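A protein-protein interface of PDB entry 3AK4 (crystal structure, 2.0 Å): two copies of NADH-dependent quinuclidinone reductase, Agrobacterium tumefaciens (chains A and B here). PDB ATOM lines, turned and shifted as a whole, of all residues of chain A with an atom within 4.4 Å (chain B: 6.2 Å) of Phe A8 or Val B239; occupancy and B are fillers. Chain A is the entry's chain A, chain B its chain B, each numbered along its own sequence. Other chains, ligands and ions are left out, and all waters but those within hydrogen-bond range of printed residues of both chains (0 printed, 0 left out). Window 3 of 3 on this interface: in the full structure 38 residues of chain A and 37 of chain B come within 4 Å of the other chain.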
ATOM      1  N   GLY A   6       5.215  14.466  -1.756  1.00  0.00           N
ATOM      2  CA  GLY A   6       4.017  14.577  -0.859  1.00  0.00           C
ATOM      3  C   GLY A   6       4.434  14.592   0.608  1.00  0.00           C
ATOM      4  O   GLY A   6       5.524  14.087   0.960  1.00  0.00           O
ATOM      5  N   ILE A   7       3.600  15.181   1.474  1.00  0.00           N
ATOM      6  CA  ILE A   7       3.921  15.165   2.907  1.00  0.00           C
ATOM      7  C   ILE A   7       3.683  13.804   3.565  1.00  0.00           C
ATOM      8  O   ILE A   7       4.098  13.630   4.699  1.00  0.00           O
ATOM      9  CB  ILE A   7       3.273  16.313   3.796  1.00  0.00           C
ATOM     10  CG1 ILE A   7       1.972  16.824   3.204  1.00  0.00           C
ATOM     11  CG2 ILE A   7       4.332  17.445   4.155  1.00  0.00           C
ATOM     12  CD1 ILE A   7       0.822  15.949   3.474  1.00  0.00           C
ATOM     13  N   PHE A   8       3.000  12.878   2.875  1.00  0.00           N
ATOM     14  CA  PHE A   8       2.825  11.498   3.372  1.00  0.00           C
ATOM     15  C   PHE A   8       3.899  10.502   2.908  1.00  0.00           C
ATOM     16  O   PHE A   8       3.879   9.339   3.291  1.00  0.00           O
ATOM     17  CB  PHE A   8       1.427  10.945   3.071  1.00  0.00           C
ATOM     18  CG  PHE A   8       0.306  11.826   3.554  1.00  0.00           C
ATOM     19  CD1 PHE A   8      -0.115  11.786   4.883  1.00  0.00           C
ATOM     20  CD2 PHE A   8      -0.305  12.724   2.678  1.00  0.00           C
ATOM     21  CE1 PHE A   8      -1.158  12.607   5.333  1.00  0.00           C
ATOM     22  CE2 PHE A   8      -1.340  13.559   3.119  1.00  0.00           C
ATOM     23  CZ  PHE A   8      -1.762  13.502   4.453  1.00  0.00           C
ATOM     24  N   ASP A   9       4.849  10.983   2.124  1.00  0.00           N
ATOM     25  CA  ASP A   9       5.905  10.156   1.517  1.00  0.00           C
ATOM     26  C   ASP A   9       7.031   9.789   2.514  1.00  0.00           C
ATOM     27  O   ASP A   9       7.542  10.656   3.219  1.00  0.00           O
ATOM     28  CB  ASP A   9       6.450  10.918   0.301  1.00  0.00           C
ATOM     29  CG  ASP A   9       7.530  10.163  -0.456  1.00  0.00           C
ATOM     30  OD1 ASP A   9       7.562   8.927  -0.450  1.00  0.00           O
ATOM     31  OD2 ASP A   9       8.355  10.844  -1.104  1.00  0.00           O
ATOM     32  N   LEU A  10       7.401   8.502   2.578  1.00  0.00           N
ATOM     33  CA  LEU A  10       8.529   8.057   3.415  1.00  0.00           C
ATOM     34  C   LEU A  10       9.742   7.584   2.574  1.00  0.00           C
ATOM     35  O   LEU A  10      10.616   6.858   3.080  1.00  0.00           O
ATOM     36  CB  LEU A  10       8.074   6.954   4.379  1.00  0.00           C
ATOM     37  CG  LEU A  10       6.861   7.237   5.288  1.00  0.00           C
ATOM     38  CD1 LEU A  10       6.614   5.953   6.123  1.00  0.00           C
ATOM     39  CD2 LEU A  10       7.119   8.428   6.201  1.00  0.00           C
ATOM     40  N   PHE A 240       0.739   7.437   8.800  1.00  0.00           N
ATOM     41  CA  PHE A 240       0.463   8.856   9.048  1.00  0.00           C
ATOM     42  C   PHE A 240       1.386   9.411  10.144  1.00  0.00           C
ATOM     43  O   PHE A 240       2.082  10.453   9.950  1.00  0.00           O
ATOM     44  CB  PHE A 240      -1.006   9.051   9.461  1.00  0.00           C
ATOM     45  CG  PHE A 240      -1.266  10.382  10.109  1.00  0.00           C
ATOM     46  CD1 PHE A 240      -1.106  11.576   9.383  1.00  0.00           C
ATOM     47  CD2 PHE A 240      -1.682  10.450  11.448  1.00  0.00           C
ATOM     48  CE1 PHE A 240      -1.318  12.836  10.011  1.00  0.00           C
ATOM     49  CE2 PHE A 240      -1.933  11.698  12.058  1.00  0.00           C
ATOM     50  CZ  PHE A 240      -1.740  12.883  11.338  1.00  0.00           C
ATOM     51  N   SER A 243       4.913   9.944   9.275  1.00  0.00           N
ATOM     52  CA  SER A 243       5.089  10.940   8.198  1.00  0.00           C
ATOM     53  C   SER A 243       5.177  12.388   8.703  1.00  0.00           C
ATOM     54  O   SER A 243       4.739  12.685   9.813  1.00  0.00           O
ATOM     55  CB  SER A 243       3.951  10.810   7.184  1.00  0.00           C
ATOM     56  OG  SER A 243       2.800  11.535   7.603  1.00  0.00           O
ATOM     57  N   ALA A 245       3.280  14.744   7.780  1.00  0.00           N
ATOM     58  CA  ALA A 245       1.925  15.279   8.057  1.00  0.00           C
ATOM     59  C   ALA A 245       1.610  15.361   9.567  1.00  0.00           C
ATOM     60  O   ALA A 245       0.816  16.229  10.005  1.00  0.00           O
ATOM     61  CB  ALA A 245       0.848  14.464   7.342  1.00  0.00           C
ATOM     62  N   PHE B   8      -3.961   8.012   0.991  1.00  0.00           N
ATOM     63  CA  PHE B   8      -4.102   9.429   1.380  1.00  0.00           C
ATOM     64  C   PHE B   8      -4.739  10.315   0.277  1.00  0.00           C
ATOM     65  O   PHE B   8      -4.983  11.503   0.512  1.00  0.00           O
ATOM     66  CB  PHE B   8      -2.764  10.042   1.868  1.00  0.00           C
ATOM     67  CG  PHE B   8      -2.151   9.316   3.030  1.00  0.00           C
ATOM     68  CD1 PHE B   8      -2.652   9.476   4.326  1.00  0.00           C
ATOM     69  CD2 PHE B   8      -1.080   8.447   2.831  1.00  0.00           C
ATOM     70  CE1 PHE B   8      -2.090   8.783   5.415  1.00  0.00           C
ATOM     71  CE2 PHE B   8      -0.504   7.748   3.915  1.00  0.00           C
ATOM     72  CZ  PHE B   8      -1.023   7.922   5.213  1.00  0.00           C
ATOM     73  N   LEU B  10      -7.326  12.169  -2.201  1.00  0.00           N
ATOM     74  CA  LEU B  10      -8.713  12.678  -2.217  1.00  0.00           C
ATOM     75  C   LEU B  10      -9.293  12.971  -3.645  1.00  0.00           C
ATOM     76  O   LEU B  10     -10.304  13.701  -3.799  1.00  0.00           O
ATOM     77  CB  LEU B  10      -8.847  13.924  -1.304  1.00  0.00           C
ATOM     78  CG  LEU B  10      -8.474  13.820   0.187  1.00  0.00           C
ATOM     79  CD1 LEU B  10      -8.665  15.188   0.897  1.00  0.00           C
ATOM     80  CD2 LEU B  10      -9.241  12.697   0.959  1.00  0.00           C
ATOM     81  N   ILE B  28      -6.610  24.616   5.144  1.00  0.00           N
ATOM     82  CA  ILE B  28      -7.370  23.372   4.923  1.00  0.00           C
ATOM     83  C   ILE B  28      -7.819  23.247   3.454  1.00  0.00           C
ATOM     84  O   ILE B  28      -7.579  22.222   2.799  1.00  0.00           O
ATOM     85  CB  ILE B  28      -8.568  23.297   5.915  1.00  0.00           C
ATOM     86  CG1 ILE B  28      -8.070  23.064   7.352  1.00  0.00           C
ATOM     87  CG2 ILE B  28      -9.581  22.235   5.536  1.00  0.00           C
ATOM     88  CD1 ILE B  28      -9.232  23.172   8.415  1.00  0.00           C
ATOM     89  N   ALA B  31      -4.899  22.491   1.171  1.00  0.00           N
ATOM     90  CA  ALA B  31      -4.360  21.152   1.391  1.00  0.00           C
ATOM     91  C   ALA B  31      -5.278  20.025   0.841  1.00  0.00           C
ATOM     92  O   ALA B  31      -4.794  18.990   0.343  1.00  0.00           O
ATOM     93  CB  ALA B  31      -4.056  20.968   2.919  1.00  0.00           C
ATOM     94  N   LEU B  32      -6.592  20.220   0.933  1.00  0.00           N
ATOM     95  CA  LEU B  32      -7.553  19.269   0.396  1.00  0.00           C
ATOM     96  C   LEU B  32      -7.472  19.218  -1.120  1.00  0.00           C
ATOM     97  O   LEU B  32      -7.455  18.114  -1.719  1.00  0.00           O
ATOM     98  CB  LEU B  32      -8.995  19.616   0.827  1.00  0.00           C
ATOM     99  CG  LEU B  32      -9.432  19.499   2.307  1.00  0.00           C
ATOM    100  CD1 LEU B  32     -10.832  20.050   2.489  1.00  0.00           C
ATOM    101  CD2 LEU B  32      -9.335  18.100   2.894  1.00  0.00           C
ATOM    102  N   ALA B  35      -4.427  17.478  -2.301  1.00  0.00           N
ATOM    103  CA  ALA B  35      -4.647  16.037  -2.127  1.00  0.00           C
ATOM    104  C   ALA B  35      -5.579  15.457  -3.206  1.00  0.00           C
ATOM    105  O   ALA B  35      -5.735  14.224  -3.323  1.00  0.00           O
ATOM    106  CB  ALA B  35      -5.191  15.749  -0.685  1.00  0.00           C
ATOM    107  N   VAL B 234      -1.894  22.170  11.081  1.00  0.00           N
ATOM    108  CA  VAL B 234      -3.274  21.678  11.278  1.00  0.00           C
ATOM    109  C   VAL B 234      -3.857  21.079   9.988  1.00  0.00           C
ATOM    110  O   VAL B 234      -4.383  19.978  10.004  1.00  0.00           O
ATOM    111  CB  VAL B 234      -4.238  22.805  11.760  1.00  0.00           C
ATOM    112  CG1 VAL B 234      -5.667  22.217  11.998  1.00  0.00           C
ATOM    113  CG2 VAL B 234      -3.722  23.454  13.042  1.00  0.00           C
ATOM    114  N   ALA B 235      -3.768  21.825   8.878  1.00  0.00           N
ATOM    115  CA  ALA B 235      -4.373  21.413   7.595  1.00  0.00           C
ATOM    116  C   ALA B 235      -3.946  20.025   7.128  1.00  0.00           C
ATOM    117  O   ALA B 235      -4.734  19.338   6.508  1.00  0.00           O
ATOM    118  CB  ALA B 235      -4.048  22.455   6.484  1.00  0.00           C
ATOM    119  N   ASP B 236      -2.692  19.623   7.381  1.00  0.00           N
ATOM    120  CA  ASP B 236      -2.211  18.323   6.847  1.00  0.00           C
ATOM    121  C   ASP B 236      -2.827  17.144   7.636  1.00  0.00           C
ATOM    122  O   ASP B 236      -3.067  16.045   7.076  1.00  0.00           O
ATOM    123  CB  ASP B 236      -0.665  18.289   6.800  1.00  0.00           C
ATOM    124  CG  ASP B 236      -0.083  19.256   5.744  1.00  0.00           C
ATOM    125  OD1 ASP B 236      -0.831  19.625   4.809  1.00  0.00           O
ATOM    126  OD2 ASP B 236       1.115  19.637   5.845  1.00  0.00           O
ATOM    127  N   VAL B 237      -3.087  17.401   8.929  1.00  0.00           N
ATOM    128  CA  VAL B 237      -3.857  16.461   9.783  1.00  0.00           C
ATOM    129  C   VAL B 237      -5.324  16.316   9.332  1.00  0.00           C
ATOM    130  O   VAL B 237      -5.865  15.204   9.279  1.00  0.00           O
ATOM    131  CB  VAL B 237      -3.778  16.827  11.294  1.00  0.00           C
ATOM    132  CG1 VAL B 237      -4.468  15.740  12.167  1.00  0.00           C
ATOM    133  CG2 VAL B 237      -2.306  16.960  11.723  1.00  0.00           C
ATOM    134  N   VAL B 238      -5.965  17.439   9.027  1.00  0.00           N
ATOM    135  CA  VAL B 238      -7.335  17.428   8.458  1.00  0.00           C
ATOM    136  C   VAL B 238      -7.397  16.592   7.155  1.00  0.00           C
ATOM    137  O   VAL B 238      -8.360  15.833   6.948  1.00  0.00           O
ATOM    138  CB  VAL B 238      -7.883  18.875   8.206  1.00  0.00           C
ATOM    139  CG1 VAL B 238      -9.301  18.832   7.619  1.00  0.00           C
ATOM    140  CG2 VAL B 238      -7.870  19.687   9.506  1.00  0.00           C
ATOM    141  N   VAL B 239      -6.376  16.716   6.300  1.00  0.00           N
ATOM    142  CA  VAL B 239      -6.298  15.865   5.091  1.00  0.00           C
ATOM    143  C   VAL B 239      -6.303  14.363   5.472  1.00  0.00           C
ATOM    144  O   VAL B 239      -7.042  13.585   4.904  1.00  0.00           O
ATOM    145  CB  VAL B 239      -5.081  16.207   4.176  1.00  0.00           C
ATOM    146  CG1 VAL B 239      -4.928  15.149   3.074  1.00  0.00           C
ATOM    147  CG2 VAL B 239      -5.229  17.610   3.552  1.00  0.00           C
ATOM    148  N   PHE B 240      -5.489  13.985   6.456  1.00  0.00           N
ATOM    149  CA  PHE B 240      -5.477  12.593   6.956  1.00  0.00           C
ATOM    150  C   PHE B 240      -6.879  12.130   7.445  1.00  0.00           C
ATOM    151  O   PHE B 240      -7.386  11.076   7.041  1.00  0.00           O
ATOM    152  CB  PHE B 240      -4.415  12.429   8.074  1.00  0.00           C
ATOM    153  CG  PHE B 240      -4.629  11.185   8.919  1.00  0.00           C
ATOM    154  CD1 PHE B 240      -4.346   9.912   8.400  1.00  0.00           C
ATOM    155  CD2 PHE B 240      -5.132  11.293  10.210  1.00  0.00           C
ATOM    156  CE1 PHE B 240      -4.559   8.745   9.179  1.00  0.00           C
ATOM    157  CE2 PHE B 240      -5.355  10.154  11.008  1.00  0.00           C
ATOM    158  CZ  PHE B 240      -5.084   8.871  10.483  1.00  0.00           C
ATOM    159  N   LEU B 241      -7.530  12.957   8.259  1.00  0.00           N
ATOM    160  CA  LEU B 241      -8.832  12.611   8.850  1.00  0.00           C
ATOM    161  C   LEU B 241      -9.953  12.495   7.797  1.00  0.00           C
ATOM    162  O   LEU B 241     -10.903  11.711   7.951  1.00  0.00           O
ATOM    163  CB  LEU B 241      -9.187  13.632   9.961  1.00  0.00           C
ATOM    164  CG  LEU B 241      -8.341  13.489  11.245  1.00  0.00           C
ATOM    165  CD1 LEU B 241      -8.621  14.638  12.300  1.00  0.00           C
ATOM    166  CD2 LEU B 241      -8.575  12.087  11.910  1.00  0.00           C
ATOM    167  N   ALA B 242      -9.816  13.265   6.720  1.00  0.00           N
ATOM    168  CA  ALA B 242     -10.720  13.200   5.572  1.00  0.00           C
ATOM    169  C   ALA B 242     -10.518  11.940   4.695  1.00  0.00           C
ATOM    170  O   ALA B 242     -11.473  11.485   4.016  1.00  0.00           O
ATOM    171  CB  ALA B 242     -10.542  14.468   4.714  1.00  0.00           C
ATOM    172  N   SER B 243      -9.296  11.394   4.699  1.00  0.00           N
ATOM    173  CA  SER B 243      -8.882  10.299   3.778  1.00  0.00           C
ATOM    174  C   SER B 243      -9.222   8.896   4.285  1.00  0.00           C
ATOM    175  O   SER B 243      -9.524   8.706   5.466  1.00  0.00           O
ATOM    176  CB  SER B 243      -7.382  10.383   3.476  1.00  0.00           C
ATOM    177  OG  SER B 243      -6.645   9.835   4.563  1.00  0.00           O
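Phe A8 touches just these residues of chain B: Phe B8, Asp B236 and Val B239.
Val B239 touches just one residue of chain A: Phe A8.
Of the printed residues of chain B, Phe A240 touches Phe B240.
Printed residues of chain B within 4 Å of Ile A7: Asp B236.
Of the printed residues of chain A, Phe B240 touches Phe A240.
Gly A6 touches none of the printed residues of chain B.
The nearest printed residue of chain A that does not touch Val B239 is Ile A7 (5.8 Å).
The nearest printed residue of chain B that does not touch Phe A240 is Phe B8 (4.03 Å).
The backbone NH (N) of Ala A245 is in hydrogen-bond range of the backbone carbonyl oxygen (O) of Ile A7 (3.4 Å).
O of Phe A240 sits at hydrogen-bond distance from OG of Ser A243 (2.7 Å).
OG of Ser A243 sits close to N of Ala A245 (3.2 Å).
OG of Ser B243 is in hydrogen-bond range of O of Phe B240 (2.9 Å).
Among the printed residues, merely in contact across the chains: Ile A7 with Asp B236, Phe A8 with Phe B8, Phe A8 with Asp B236, Phe A8 with Val B239, Phe A240 with Phe B240 and Ala A245 with Val B237.
Of the 8 printed residues of chain A, 4 touch a printed residue of chain B.
Printed residues of chain A that touch a printed residue of chain B: Ile A7, Phe A8, Phe A240 and Ala A245.
Printed residues of chain B that touch a printed residue of chain A: Phe B8, Asp B236, Val B237, Val B239 and Phe B240.
Among the printed residues, no Asp or Glu carboxylate lies within 4 Å of a Lys or Arg side-chain nitrogen of the other chain.
Phe A8 touches its own counterpart, Phe B8.
Phe A240 touches its own counterpart, Phe B240.
Of the 6 pairs that touch across the chains among the printed residues, 2 have their exchanged pair printed and touching as well.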
